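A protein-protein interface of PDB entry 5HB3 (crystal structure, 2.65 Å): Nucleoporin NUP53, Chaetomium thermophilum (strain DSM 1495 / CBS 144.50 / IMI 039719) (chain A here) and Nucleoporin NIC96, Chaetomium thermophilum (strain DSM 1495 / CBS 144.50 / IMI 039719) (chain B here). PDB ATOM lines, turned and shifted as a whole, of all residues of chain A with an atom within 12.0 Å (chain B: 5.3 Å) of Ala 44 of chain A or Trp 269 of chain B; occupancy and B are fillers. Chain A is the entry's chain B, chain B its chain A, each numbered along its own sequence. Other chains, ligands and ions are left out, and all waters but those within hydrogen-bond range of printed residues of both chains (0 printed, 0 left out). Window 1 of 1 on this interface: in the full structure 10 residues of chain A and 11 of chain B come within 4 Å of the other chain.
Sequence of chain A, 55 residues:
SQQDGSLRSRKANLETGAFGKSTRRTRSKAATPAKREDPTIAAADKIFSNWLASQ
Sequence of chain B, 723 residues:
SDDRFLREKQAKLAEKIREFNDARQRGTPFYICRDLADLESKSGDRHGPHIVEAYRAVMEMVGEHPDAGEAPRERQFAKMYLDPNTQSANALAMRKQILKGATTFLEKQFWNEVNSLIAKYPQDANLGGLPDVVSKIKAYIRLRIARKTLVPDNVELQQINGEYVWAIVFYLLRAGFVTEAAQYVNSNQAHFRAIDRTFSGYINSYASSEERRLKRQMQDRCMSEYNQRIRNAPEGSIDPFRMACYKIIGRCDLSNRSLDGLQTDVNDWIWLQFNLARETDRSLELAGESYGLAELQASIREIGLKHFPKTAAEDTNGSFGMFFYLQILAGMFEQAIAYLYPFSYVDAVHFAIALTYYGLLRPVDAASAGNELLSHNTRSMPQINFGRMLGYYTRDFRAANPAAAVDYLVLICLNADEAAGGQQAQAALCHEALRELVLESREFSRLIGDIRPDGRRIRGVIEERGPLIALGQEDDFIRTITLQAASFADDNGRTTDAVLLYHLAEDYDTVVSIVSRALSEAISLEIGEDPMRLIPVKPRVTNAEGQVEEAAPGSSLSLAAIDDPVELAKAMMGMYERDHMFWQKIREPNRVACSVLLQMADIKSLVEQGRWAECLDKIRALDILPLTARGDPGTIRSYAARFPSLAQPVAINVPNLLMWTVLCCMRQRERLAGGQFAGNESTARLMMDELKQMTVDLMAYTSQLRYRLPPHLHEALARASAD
The side-chain carboxylate (OD1) of Asp 45 of chain A is in hydrogen-bond range of a ring nitrogen (NE2) of His 307 of chain B, at 3.0 Å.
The guanidinium group of Arg 257 of chain B lies within hydrogen-bond range of the side-chain amide oxygen of Gln 273 of chain B (2.8 Å). NE1 of Trp 269 of chain B sits close to NE2 of Gln 273 of chain B (3.1 Å). The side-chain hydroxyl (OG) of Ser 49 of chain A lies within hydrogen-bond range of the backbone carbonyl oxygen (O) of Asp 45 of chain A (2.8 Å).
Arg 257 of chain B touches Thr 40 of chain A (N to CB, 3.6 Å). Trp 269 of chain B touches Ala 44 of chain A. Ile 47 of chain A touches Trp 269 of chain B. CG2 of Val 266 of chain B touches CE1 of Phe 48 of chain A, at 3.9 Å. CE2 of Phe 48 of chain A touches CZ3 of Trp 269 of chain B (3.7 Å). Phe 48 of chain A touches Ile 303 of chain B (CE2 to CD1, 3.3 Å). CB of Phe 48 of chain A touches ND1 of His 307 of chain B, 3.9 Å away. Leu 326 of chain B touches Phe 48 of chain A. Ser 49 of chain A touches His 307 of chain B. CG1 of Val 266 of chain B touches CD1 of Trp 51 of chain A, 3.8 Å away.
Printed residues of chain B within 4 Å of Thr 40 of chain A: Arg 257. Ala 44 of chain A touches just one residue of chain B: Trp 269 (3.8 Å). Of the printed residues of chain B, Asp 45 of chain A touches His 307 (3.0 Å). Printed residues of chain B within 4 Å of Ile 47 of chain A: Trp 269. Printed residues of chain B within 4 Å of Trp 51 of chain A: Val 266. No residue of chain A comes within 4 Å of Asp 265 of chain B. No residue of chain A comes within 4 Å of Asn 267 of chain B. No residue of chain A comes within 4 Å of Asp 268 of chain B. No residue of chain A comes within 4 Å of Ile 270 of chain B. Trp 271 of chain B touches none of the printed residues of chain A. No residue of chain A comes within 4 Å of Ser 299 of chain B. No residue of chain A comes within 4 Å of Ile 300 of chain B.
Of the 16 printed residues of chain A, 8 touch a printed residue of chain B. Printed residues of chain A that touch a printed residue of chain B: Thr 40, Ala 44, Asp 45, Ile 47, Phe 48, Ser 49, Trp 51 and Leu 52. Hydrophobic or aromatic side chains of chain A within 4 Å of the printed part of chain B: Ala 44, Ile 47, Phe 48, Trp 51 and Leu 52. Of the 16 printed residues of chain B, 6 touch a printed residue of chain A. Along chain B the printed residues that touch a printed residue of chain A span positions 257 to 326. Among the printed residues, 12 pairs touch across the chains.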
ATOM      1  N   ASP A  38     -36.719 -19.055 -12.976  1.00  0.00           N
ATOM      2  CA  ASP A  38     -36.374 -17.724 -12.484  1.00  0.00           C
ATOM      3  C   ASP A  38     -34.865 -17.481 -12.495  1.00  0.00           C
ATOM      4  O   ASP A  38     -34.412 -16.435 -12.943  1.00  0.00           O
ATOM      5  CB  ASP A  38     -36.926 -17.516 -11.069  1.00  0.00           C
ATOM      6  CG  ASP A  38     -37.560 -16.148 -10.886  1.00  0.00           C
ATOM      7  OD1 ASP A  38     -37.461 -15.592  -9.770  1.00  0.00           O
ATOM      8  OD2 ASP A  38     -38.161 -15.630 -11.853  1.00  0.00           O
ATOM      9  N   PRO A  39     -34.078 -18.444 -11.996  1.00  0.00           N
ATOM     10  CA  PRO A  39     -32.621 -18.283 -11.981  1.00  0.00           C
ATOM     11  C   PRO A  39     -32.044 -18.199 -13.389  1.00  0.00           C
ATOM     12  O   PRO A  39     -31.157 -17.386 -13.648  1.00  0.00           O
ATOM     13  CB  PRO A  39     -32.132 -19.548 -11.260  1.00  0.00           C
ATOM     14  CG  PRO A  39     -33.321 -20.037 -10.488  1.00  0.00           C
ATOM     15  CD  PRO A  39     -34.499 -19.699 -11.354  1.00  0.00           C
ATOM     16  N   THR A  40     -32.551 -19.035 -14.290  1.00  0.00           N
ATOM     17  CA  THR A  40     -32.106 -19.017 -15.680  1.00  0.00           C
ATOM     18  C   THR A  40     -32.497 -17.713 -16.366  1.00  0.00           C
ATOM     19  O   THR A  40     -31.742 -17.179 -17.180  1.00  0.00           O
ATOM     20  CB  THR A  40     -32.685 -20.204 -16.490  1.00  0.00           C
ATOM     21  OG1 THR A  40     -32.264 -20.102 -17.857  1.00  0.00           O
ATOM     22  CG2 THR A  40     -34.212 -20.223 -16.434  1.00  0.00           C
ATOM     23  N   ILE A  41     -33.678 -17.205 -16.033  1.00  0.00           N
ATOM     24  CA  ILE A  41     -34.174 -15.978 -16.643  1.00  0.00           C
ATOM     25  C   ILE A  41     -33.397 -14.793 -16.082  1.00  0.00           C
ATOM     26  O   ILE A  41     -33.043 -13.866 -16.813  1.00  0.00           O
ATOM     27  CB  ILE A  41     -35.680 -15.759 -16.377  1.00  0.00           C
ATOM     28  CG1 ILE A  41     -36.477 -17.048 -16.617  1.00  0.00           C
ATOM     29  CG2 ILE A  41     -36.211 -14.644 -17.269  1.00  0.00           C
ATOM     30  CD1 ILE A  41     -37.871 -17.017 -16.034  1.00  0.00           C
ATOM     31  N   ALA A  42     -33.131 -14.835 -14.781  1.00  0.00           N
ATOM     32  CA  ALA A  42     -32.383 -13.779 -14.112  1.00  0.00           C
ATOM     33  C   ALA A  42     -30.922 -13.804 -14.548  1.00  0.00           C
ATOM     34  O   ALA A  42     -30.241 -12.779 -14.525  1.00  0.00           O
ATOM     35  CB  ALA A  42     -32.489 -13.937 -12.603  1.00  0.00           C
ATOM     36  N   ALA A  43     -30.447 -14.981 -14.945  1.00  0.00           N
ATOM     37  CA  ALA A  43     -29.068 -15.141 -15.387  1.00  0.00           C
ATOM     38  C   ALA A  43     -28.897 -14.666 -16.825  1.00  0.00           C
ATOM     39  O   ALA A  43     -27.895 -14.040 -17.163  1.00  0.00           O
ATOM     40  CB  ALA A  43     -28.640 -16.595 -15.255  1.00  0.00           C
ATOM     41  N   ALA A  44     -29.876 -14.969 -17.671  1.00  0.00           N
ATOM     42  CA  ALA A  44     -29.841 -14.534 -19.063  1.00  0.00           C
ATOM     43  C   ALA A  44     -29.774 -13.012 -19.140  1.00  0.00           C
ATOM     44  O   ALA A  44     -28.996 -12.452 -19.911  1.00  0.00           O
ATOM     45  CB  ALA A  44     -31.061 -15.050 -19.811  1.00  0.00           C
ATOM     46  N   ASP A  45     -30.594 -12.349 -18.329  1.00  0.00           N
ATOM     47  CA  ASP A  45     -30.606 -10.892 -18.267  1.00  0.00           C
ATOM     48  C   ASP A  45     -29.215 -10.355 -17.943  1.00  0.00           C
ATOM     49  O   ASP A  45     -28.798  -9.323 -18.468  1.00  0.00           O
ATOM     50  CB  ASP A  45     -31.605 -10.416 -17.210  1.00  0.00           C
ATOM     51  CG  ASP A  45     -33.025 -10.851 -17.512  1.00  0.00           C
ATOM     52  OD1 ASP A  45     -33.411 -10.839 -18.700  1.00  0.00           O
ATOM     53  OD2 ASP A  45     -33.752 -11.207 -16.561  1.00  0.00           O
ATOM     54  N   LYS A  46     -28.504 -11.067 -17.074  1.00  0.00           N
ATOM     55  CA  LYS A  46     -27.165 -10.667 -16.658  1.00  0.00           C
ATOM     56  C   LYS A  46     -26.170 -10.762 -17.814  1.00  0.00           C
ATOM     57  O   LYS A  46     -25.290  -9.914 -17.959  1.00  0.00           O
ATOM     58  CB  LYS A  46     -26.698 -11.552 -15.499  1.00  0.00           C
ATOM     59  CG  LYS A  46     -25.290 -11.260 -14.999  1.00  0.00           C
ATOM     60  CD  LYS A  46     -24.487 -12.544 -14.828  1.00  0.00           C
ATOM     61  CE  LYS A  46     -23.899 -12.659 -13.432  1.00  0.00           C
ATOM     62  NZ  LYS A  46     -23.145 -13.932 -13.255  1.00  0.00           N
ATOM     63  N   ILE A  47     -26.320 -11.797 -18.636  1.00  0.00           N
ATOM     64  CA  ILE A  47     -25.368 -12.072 -19.708  1.00  0.00           C
ATOM     65  C   ILE A  47     -25.581 -11.172 -20.923  1.00  0.00           C
ATOM     66  O   ILE A  47     -24.621 -10.786 -21.590  1.00  0.00           O
ATOM     67  CB  ILE A  47     -25.447 -13.547 -20.151  1.00  0.00           C
ATOM     68  CG1 ILE A  47     -25.039 -14.462 -18.994  1.00  0.00           C
ATOM     69  CG2 ILE A  47     -24.552 -13.792 -21.360  1.00  0.00           C
ATOM     70  CD1 ILE A  47     -25.209 -15.935 -19.286  1.00  0.00           C
ATOM     71  N   PHE A  48     -26.836 -10.842 -21.212  1.00  0.00           N
ATOM     72  CA  PHE A  48     -27.149 -10.007 -22.366  1.00  0.00           C
ATOM     73  C   PHE A  48     -26.995  -8.519 -22.056  1.00  0.00           C
ATOM     74  O   PHE A  48     -26.512  -7.758 -22.893  1.00  0.00           O
ATOM     75  CB  PHE A  48     -28.554 -10.308 -22.890  1.00  0.00           C
ATOM     76  CG  PHE A  48     -28.632 -11.569 -23.703  1.00  0.00           C
ATOM     77  CD1 PHE A  48     -28.154 -11.599 -25.001  1.00  0.00           C
ATOM     78  CD2 PHE A  48     -29.176 -12.724 -23.169  1.00  0.00           C
ATOM     79  CE1 PHE A  48     -28.218 -12.758 -25.752  1.00  0.00           C
ATOM     80  CE2 PHE A  48     -29.242 -13.885 -23.915  1.00  0.00           C
ATOM     81  CZ  PHE A  48     -28.764 -13.902 -25.208  1.00  0.00           C
ATOM     82  N   SER A  49     -27.399  -8.107 -20.857  1.00  0.00           N
ATOM     83  CA  SER A  49     -27.158  -6.739 -20.415  1.00  0.00           C
ATOM     84  C   SER A  49     -25.663  -6.455 -20.477  1.00  0.00           C
ATOM     85  O   SER A  49     -25.234  -5.420 -20.988  1.00  0.00           O
ATOM     86  CB  SER A  49     -27.671  -6.526 -18.989  1.00  0.00           C
ATOM     87  OG  SER A  49     -29.087  -6.565 -18.941  1.00  0.00           O
ATOM     88  N   ASN A  50     -24.876  -7.390 -19.956  1.00  0.00           N
ATOM     89  CA  ASN A  50     -23.424  -7.288 -19.989  1.00  0.00           C
ATOM     90  C   ASN A  50     -22.884  -7.284 -21.417  1.00  0.00           C
ATOM     91  O   ASN A  50     -21.904  -6.601 -21.717  1.00  0.00           O
ATOM     92  CB  ASN A  50     -22.802  -8.439 -19.194  1.00  0.00           C
ATOM     93  CG  ASN A  50     -21.317  -8.594 -19.452  1.00  0.00           C
ATOM     94  OD1 ASN A  50     -20.493  -7.911 -18.842  1.00  0.00           O
ATOM     95  ND2 ASN A  50     -20.965  -9.502 -20.354  1.00  0.00           N
ATOM     96  N   TRP A  51     -23.528  -8.046 -22.295  1.00  0.00           N
ATOM     97  CA  TRP A  51     -23.097  -8.146 -23.685  1.00  0.00           C
ATOM     98  C   TRP A  51     -23.402  -6.863 -24.456  1.00  0.00           C
ATOM     99  O   TRP A  51     -22.588  -6.403 -25.255  1.00  0.00           O
ATOM    100  CB  TRP A  51     -23.773  -9.339 -24.365  1.00  0.00           C
ATOM    101  CG  TRP A  51     -23.391  -9.510 -25.807  1.00  0.00           C
ATOM    102  CD1 TRP A  51     -22.347 -10.237 -26.299  1.00  0.00           C
ATOM    103  CD2 TRP A  51     -24.056  -8.944 -26.944  1.00  0.00           C
ATOM    104  NE1 TRP A  51     -22.318 -10.158 -27.671  1.00  0.00           N
ATOM    105  CE2 TRP A  51     -23.357  -9.370 -28.091  1.00  0.00           C
ATOM    106  CE3 TRP A  51     -25.173  -8.117 -27.103  1.00  0.00           C
ATOM    107  CZ2 TRP A  51     -23.738  -8.998 -29.379  1.00  0.00           C
ATOM    108  CZ3 TRP A  51     -25.551  -7.749 -28.383  1.00  0.00           C
ATOM    109  CH2 TRP A  51     -24.836  -8.189 -29.504  1.00  0.00           C
ATOM    110  N   LEU A  52     -24.578  -6.292 -24.214  1.00  0.00           N
ATOM    111  CA  LEU A  52     -24.978  -5.052 -24.873  1.00  0.00           C
ATOM    112  C   LEU A  52     -24.001  -3.929 -24.552  1.00  0.00           C
ATOM    113  O   LEU A  52     -23.618  -3.156 -25.430  1.00  0.00           O
ATOM    114  CB  LEU A  52     -26.387  -4.647 -24.438  1.00  0.00           C
ATOM    115  CG  LEU A  52     -27.543  -5.458 -25.024  1.00  0.00           C
ATOM    116  CD1 LEU A  52     -28.840  -5.118 -24.310  1.00  0.00           C
ATOM    117  CD2 LEU A  52     -27.674  -5.206 -26.519  1.00  0.00           C
ATOM    118  N   ALA A  53     -23.602  -3.845 -23.288  1.00  0.00           N
ATOM    119  CA  ALA A  53     -22.689  -2.801 -22.839  1.00  0.00           C
ATOM    120  C   ALA A  53     -21.304  -2.967 -23.462  1.00  0.00           C
ATOM    121  O   ALA A  53     -20.501  -2.033 -23.465  1.00  0.00           O
ATOM    122  CB  ALA A  53     -22.592  -2.808 -21.321  1.00  0.00           C
ATOM    123  N   ARG B 257     -30.322 -22.985 -16.436  1.00  0.00           N
ATOM    124  CA  ARG B 257     -29.436 -23.275 -17.555  1.00  0.00           C
ATOM    125  C   ARG B 257     -28.373 -22.193 -17.711  1.00  0.00           C
ATOM    126  O   ARG B 257     -28.492 -21.312 -18.561  1.00  0.00           O
ATOM    127  CB  ARG B 257     -30.250 -23.395 -18.845  1.00  0.00           C
ATOM    128  CG  ARG B 257     -31.409 -24.377 -18.747  1.00  0.00           C
ATOM    129  CD  ARG B 257     -32.194 -24.452 -20.045  1.00  0.00           C
ATOM    130  NE  ARG B 257     -32.862 -23.192 -20.363  1.00  0.00           N
ATOM    131  CZ  ARG B 257     -34.102 -22.874 -19.998  1.00  0.00           C
ATOM    132  NH1 ARG B 257     -34.839 -23.720 -19.288  1.00  0.00           N
ATOM    133  NH2 ARG B 257     -34.610 -21.699 -20.347  1.00  0.00           N
ATOM    134  N   SER B 258     -27.332 -22.268 -16.886  1.00  0.00           N
ATOM    135  CA  SER B 258     -26.226 -21.319 -16.952  1.00  0.00           C
ATOM    136  C   SER B 258     -24.940 -21.948 -16.420  1.00  0.00           C
ATOM    137  O   SER B 258     -24.971 -22.986 -15.762  1.00  0.00           O
ATOM    138  CB  SER B 258     -26.557 -20.062 -16.148  1.00  0.00           C
ATOM    139  OG  SER B 258     -26.714 -20.365 -14.773  1.00  0.00           O
ATOM    140  N   ASP B 265     -18.801 -16.888 -22.114  1.00  0.00           N
ATOM    141  CA  ASP B 265     -19.335 -15.743 -22.846  1.00  0.00           C
ATOM    142  C   ASP B 265     -20.739 -16.051 -23.366  1.00  0.00           C
ATOM    143  O   ASP B 265     -21.331 -17.068 -23.005  1.00  0.00           O
ATOM    144  CB  ASP B 265     -18.405 -15.349 -24.000  1.00  0.00           C
ATOM    145  CG  ASP B 265     -18.316 -16.414 -25.078  1.00  0.00           C
ATOM    146  OD1 ASP B 265     -19.178 -17.318 -25.107  1.00  0.00           O
ATOM    147  OD2 ASP B 265     -17.385 -16.338 -25.909  1.00  0.00           O
ATOM    148  N   VAL B 266     -21.269 -15.173 -24.213  1.00  0.00           N
ATOM    149  CA  VAL B 266     -22.638 -15.312 -24.703  1.00  0.00           C
ATOM    150  C   VAL B 266     -22.823 -16.570 -25.549  1.00  0.00           C
ATOM    151  O   VAL B 266     -23.893 -17.176 -25.543  1.00  0.00           O
ATOM    152  CB  VAL B 266     -23.074 -14.084 -25.534  1.00  0.00           C
ATOM    153  CG1 VAL B 266     -22.247 -13.975 -26.810  1.00  0.00           C
ATOM    154  CG2 VAL B 266     -24.557 -14.165 -25.860  1.00  0.00           C
ATOM    155  N   ASN B 267     -21.783 -16.960 -26.277  1.00  0.00           N
ATOM    156  CA  ASN B 267     -21.857 -18.146 -27.123  1.00  0.00           C
ATOM    157  C   ASN B 267     -21.926 -19.419 -26.290  1.00  0.00           C
ATOM    158  O   ASN B 267     -22.553 -20.401 -26.686  1.00  0.00           O
ATOM    159  CB  ASN B 267     -20.663 -18.201 -28.077  1.00  0.00           C
ATOM    160  CG  ASN B 267     -20.698 -17.095 -29.112  1.00  0.00           C
ATOM    161  OD1 ASN B 267     -19.816 -16.238 -29.153  1.00  0.00           O
ATOM    162  ND2 ASN B 267     -21.725 -17.106 -29.955  1.00  0.00           N
ATOM    163  N   ASP B 268     -21.282 -19.399 -25.129  1.00  0.00           N
ATOM    164  CA  ASP B 268     -21.343 -20.530 -24.217  1.00  0.00           C
ATOM    165  C   ASP B 268     -22.753 -20.655 -23.658  1.00  0.00           C
ATOM    166  O   ASP B 268     -23.267 -21.761 -23.488  1.00  0.00           O
ATOM    167  CB  ASP B 268     -20.327 -20.361 -23.088  1.00  0.00           C
ATOM    168  CG  ASP B 268     -18.891 -20.392 -23.586  1.00  0.00           C
ATOM    169  OD1 ASP B 268     -18.621 -21.091 -24.587  1.00  0.00           O
ATOM    170  OD2 ASP B 268     -18.035 -19.715 -22.980  1.00  0.00           O
ATOM    171  N   TRP B 269     -23.384 -19.516 -23.384  1.00  0.00           N
ATOM    172  CA  TRP B 269     -24.760 -19.512 -22.902  1.00  0.00           C
ATOM    173  C   TRP B 269     -25.698 -20.058 -23.971  1.00  0.00           C
ATOM    174  O   TRP B 269     -26.496 -20.954 -23.708  1.00  0.00           O
ATOM    175  CB  TRP B 269     -25.202 -18.103 -22.505  1.00  0.00           C
ATOM    176  CG  TRP B 269     -26.616 -18.058 -22.001  1.00  0.00           C
ATOM    177  CD1 TRP B 269     -27.030 -18.198 -20.710  1.00  0.00           C
ATOM    178  CD2 TRP B 269     -27.802 -17.872 -22.784  1.00  0.00           C
ATOM    179  NE1 TRP B 269     -28.398 -18.107 -20.637  1.00  0.00           N
ATOM    180  CE2 TRP B 269     -28.896 -17.906 -21.897  1.00  0.00           C
ATOM    181  CE3 TRP B 269     -28.045 -17.678 -24.147  1.00  0.00           C
ATOM    182  CZ2 TRP B 269     -30.212 -17.754 -22.329  1.00  0.00           C
ATOM    183  CZ3 TRP B 269     -29.350 -17.527 -24.573  1.00  0.00           C
ATOM    184  CH2 TRP B 269     -30.417 -17.565 -23.668  1.00  0.00           C
ATOM    185  N   ILE B 270     -25.599 -19.513 -25.179  1.00  0.00           N
ATOM    186  CA  ILE B 270     -26.437 -19.963 -26.281  1.00  0.00           C
ATOM    187  C   ILE B 270     -26.274 -21.467 -26.483  1.00  0.00           C
ATOM    188  O   ILE B 270     -27.258 -22.189 -26.641  1.00  0.00           O
ATOM    189  CB  ILE B 270     -26.098 -19.222 -27.590  1.00  0.00           C
ATOM    190  CG1 ILE B 270     -26.423 -17.731 -27.457  1.00  0.00           C
ATOM    191  CG2 ILE B 270     -26.875 -19.816 -28.757  1.00  0.00           C
ATOM    192  CD1 ILE B 270     -25.931 -16.887 -28.617  1.00  0.00           C
ATOM    193  N   TRP B 271     -25.030 -21.938 -26.466  1.00  0.00           N
ATOM    194  CA  TRP B 271     -24.753 -23.359 -26.660  1.00  0.00           C
ATOM    195  C   TRP B 271     -25.421 -24.215 -25.595  1.00  0.00           C
ATOM    196  O   TRP B 271     -25.966 -25.278 -25.892  1.00  0.00           O
ATOM    197  CB  TRP B 271     -23.249 -23.631 -26.648  1.00  0.00           C
ATOM    198  CG  TRP B 271     -22.935 -25.085 -26.485  1.00  0.00           C
ATOM    199  CD1 TRP B 271     -22.939 -26.038 -27.461  1.00  0.00           C
ATOM    200  CD2 TRP B 271     -22.580 -25.757 -25.271  1.00  0.00           C
ATOM    201  NE1 TRP B 271     -22.607 -27.260 -26.931  1.00  0.00           N
ATOM    202  CE2 TRP B 271     -22.382 -27.114 -25.587  1.00  0.00           C
ATOM    203  CE3 TRP B 271     -22.410 -25.341 -23.947  1.00  0.00           C
ATOM    204  CZ2 TRP B 271     -22.020 -28.059 -24.629  1.00  0.00           C
ATOM    205  CZ3 TRP B 271     -22.051 -26.280 -22.998  1.00  0.00           C
ATOM    206  CH2 TRP B 271     -21.861 -27.622 -23.343  1.00  0.00           C
ATOM    207  N   LEU B 272     -25.369 -23.755 -24.352  1.00  0.00           N
ATOM    208  CA  LEU B 272     -25.950 -24.507 -23.250  1.00  0.00           C
ATOM    209  C   LEU B 272     -27.450 -24.692 -23.457  1.00  0.00           C
ATOM    210  O   LEU B 272     -28.000 -25.752 -23.155  1.00  0.00           O
ATOM    211  CB  LEU B 272     -25.683 -23.800 -21.920  1.00  0.00           C
ATOM    212  CG  LEU B 272     -26.132 -24.566 -20.673  1.00  0.00           C
ATOM    213  CD1 LEU B 272     -25.365 -25.875 -20.533  1.00  0.00           C
ATOM    214  CD2 LEU B 272     -25.960 -23.709 -19.433  1.00  0.00           C
ATOM    215  N   GLN B 273     -28.105 -23.661 -23.983  1.00  0.00           N
ATOM    216  CA  GLN B 273     -29.549 -23.699 -24.192  1.00  0.00           C
ATOM    217  C   GLN B 273     -29.930 -24.787 -25.190  1.00  0.00           C
ATOM    218  O   GLN B 273     -30.910 -25.501 -24.996  1.00  0.00           O
ATOM    219  CB  GLN B 273     -30.062 -22.347 -24.693  1.00  0.00           C
ATOM    220  CG  GLN B 273     -29.690 -21.162 -23.817  1.00  0.00           C
ATOM    221  CD  GLN B 273     -30.018 -21.388 -22.358  1.00  0.00           C
ATOM    222  OE1 GLN B 273     -31.062 -21.944 -22.027  1.00  0.00           O
ATOM    223  NE2 GLN B 273     -29.120 -20.963 -21.476  1.00  0.00           N
ATOM    224  N   SER B 299     -38.055 -18.803 -24.661  1.00  0.00           N
ATOM    225  CA  SER B 299     -36.992 -18.098 -23.961  1.00  0.00           C
ATOM    226  C   SER B 299     -36.426 -16.980 -24.837  1.00  0.00           C
ATOM    227  O   SER B 299     -36.334 -15.831 -24.406  1.00  0.00           O
ATOM    228  CB  SER B 299     -35.886 -19.080 -23.560  1.00  0.00           C
ATOM    229  OG  SER B 299     -34.903 -18.452 -22.753  1.00  0.00           O
ATOM    230  N   ILE B 300     -36.061 -17.321 -26.069  1.00  0.00           N
ATOM    231  CA  ILE B 300     -35.493 -16.351 -27.002  1.00  0.00           C
ATOM    232  C   ILE B 300     -36.462 -15.202 -27.255  1.00  0.00           C
ATOM    233  O   ILE B 300     -36.065 -14.038 -27.316  1.00  0.00           O
ATOM    234  CB  ILE B 300     -35.146 -17.011 -28.352  1.00  0.00           C
ATOM    235  CG1 ILE B 300     -34.067 -18.083 -28.163  1.00  0.00           C
ATOM    236  CG2 ILE B 300     -34.690 -15.961 -29.362  1.00  0.00           C
ATOM    237  CD1 ILE B 300     -32.770 -17.560 -27.583  1.00  0.00           C
ATOM    238  N   ILE B 303     -36.309 -12.689 -24.518  1.00  0.00           N
ATOM    239  CA  ILE B 303     -35.041 -11.970 -24.528  1.00  0.00           C
ATOM    240  C   ILE B 303     -35.095 -10.843 -25.550  1.00  0.00           C
ATOM    241  O   ILE B 303     -34.495  -9.786 -25.357  1.00  0.00           O
ATOM    242  CB  ILE B 303     -33.859 -12.902 -24.853  1.00  0.00           C
ATOM    243  CG1 ILE B 303     -33.701 -13.948 -23.749  1.00  0.00           C
ATOM    244  CG2 ILE B 303     -32.574 -12.097 -25.017  1.00  0.00           C
ATOM    245  CD1 ILE B 303     -32.446 -14.775 -23.863  1.00  0.00           C
ATOM    246  N   HIS B 307     -34.362  -7.032 -24.339  1.00  0.00           N
ATOM    247  CA  HIS B 307     -33.003  -6.553 -24.583  1.00  0.00           C
ATOM    248  C   HIS B 307     -32.767  -5.928 -25.959  1.00  0.00           C
ATOM    249  O   HIS B 307     -31.773  -5.229 -26.155  1.00  0.00           O
ATOM    250  CB  HIS B 307     -32.009  -7.699 -24.374  1.00  0.00           C
ATOM    251  CG  HIS B 307     -32.012  -8.254 -22.985  1.00  0.00           C
ATOM    252  ND1 HIS B 307     -31.286  -7.689 -21.958  1.00  0.00           N
ATOM    253  CD2 HIS B 307     -32.652  -9.321 -22.451  1.00  0.00           C
ATOM    254  CE1 HIS B 307     -31.479  -8.384 -20.852  1.00  0.00           C
ATOM    255  NE2 HIS B 307     -32.304  -9.379 -21.124  1.00  0.00           N
ATOM    256  N   LEU B 326     -30.097 -15.344 -33.174  1.00  0.00           N
ATOM    257  CA  LEU B 326     -30.679 -16.251 -32.190  1.00  0.00           C
ATOM    258  C   LEU B 326     -31.953 -16.899 -32.719  1.00  0.00           C
ATOM    259  O   LEU B 326     -32.155 -18.105 -32.569  1.00  0.00           O
ATOM    260  CB  LEU B 326     -30.985 -15.506 -30.889  1.00  0.00           C
ATOM    261  CG  LEU B 326     -29.784 -15.182 -30.001  1.00  0.00           C
ATOM    262  CD1 LEU B 326     -30.191 -14.249 -28.871  1.00  0.00           C
ATOM    263  CD2 LEU B 326     -29.175 -16.458 -29.444  1.00  0.00           C
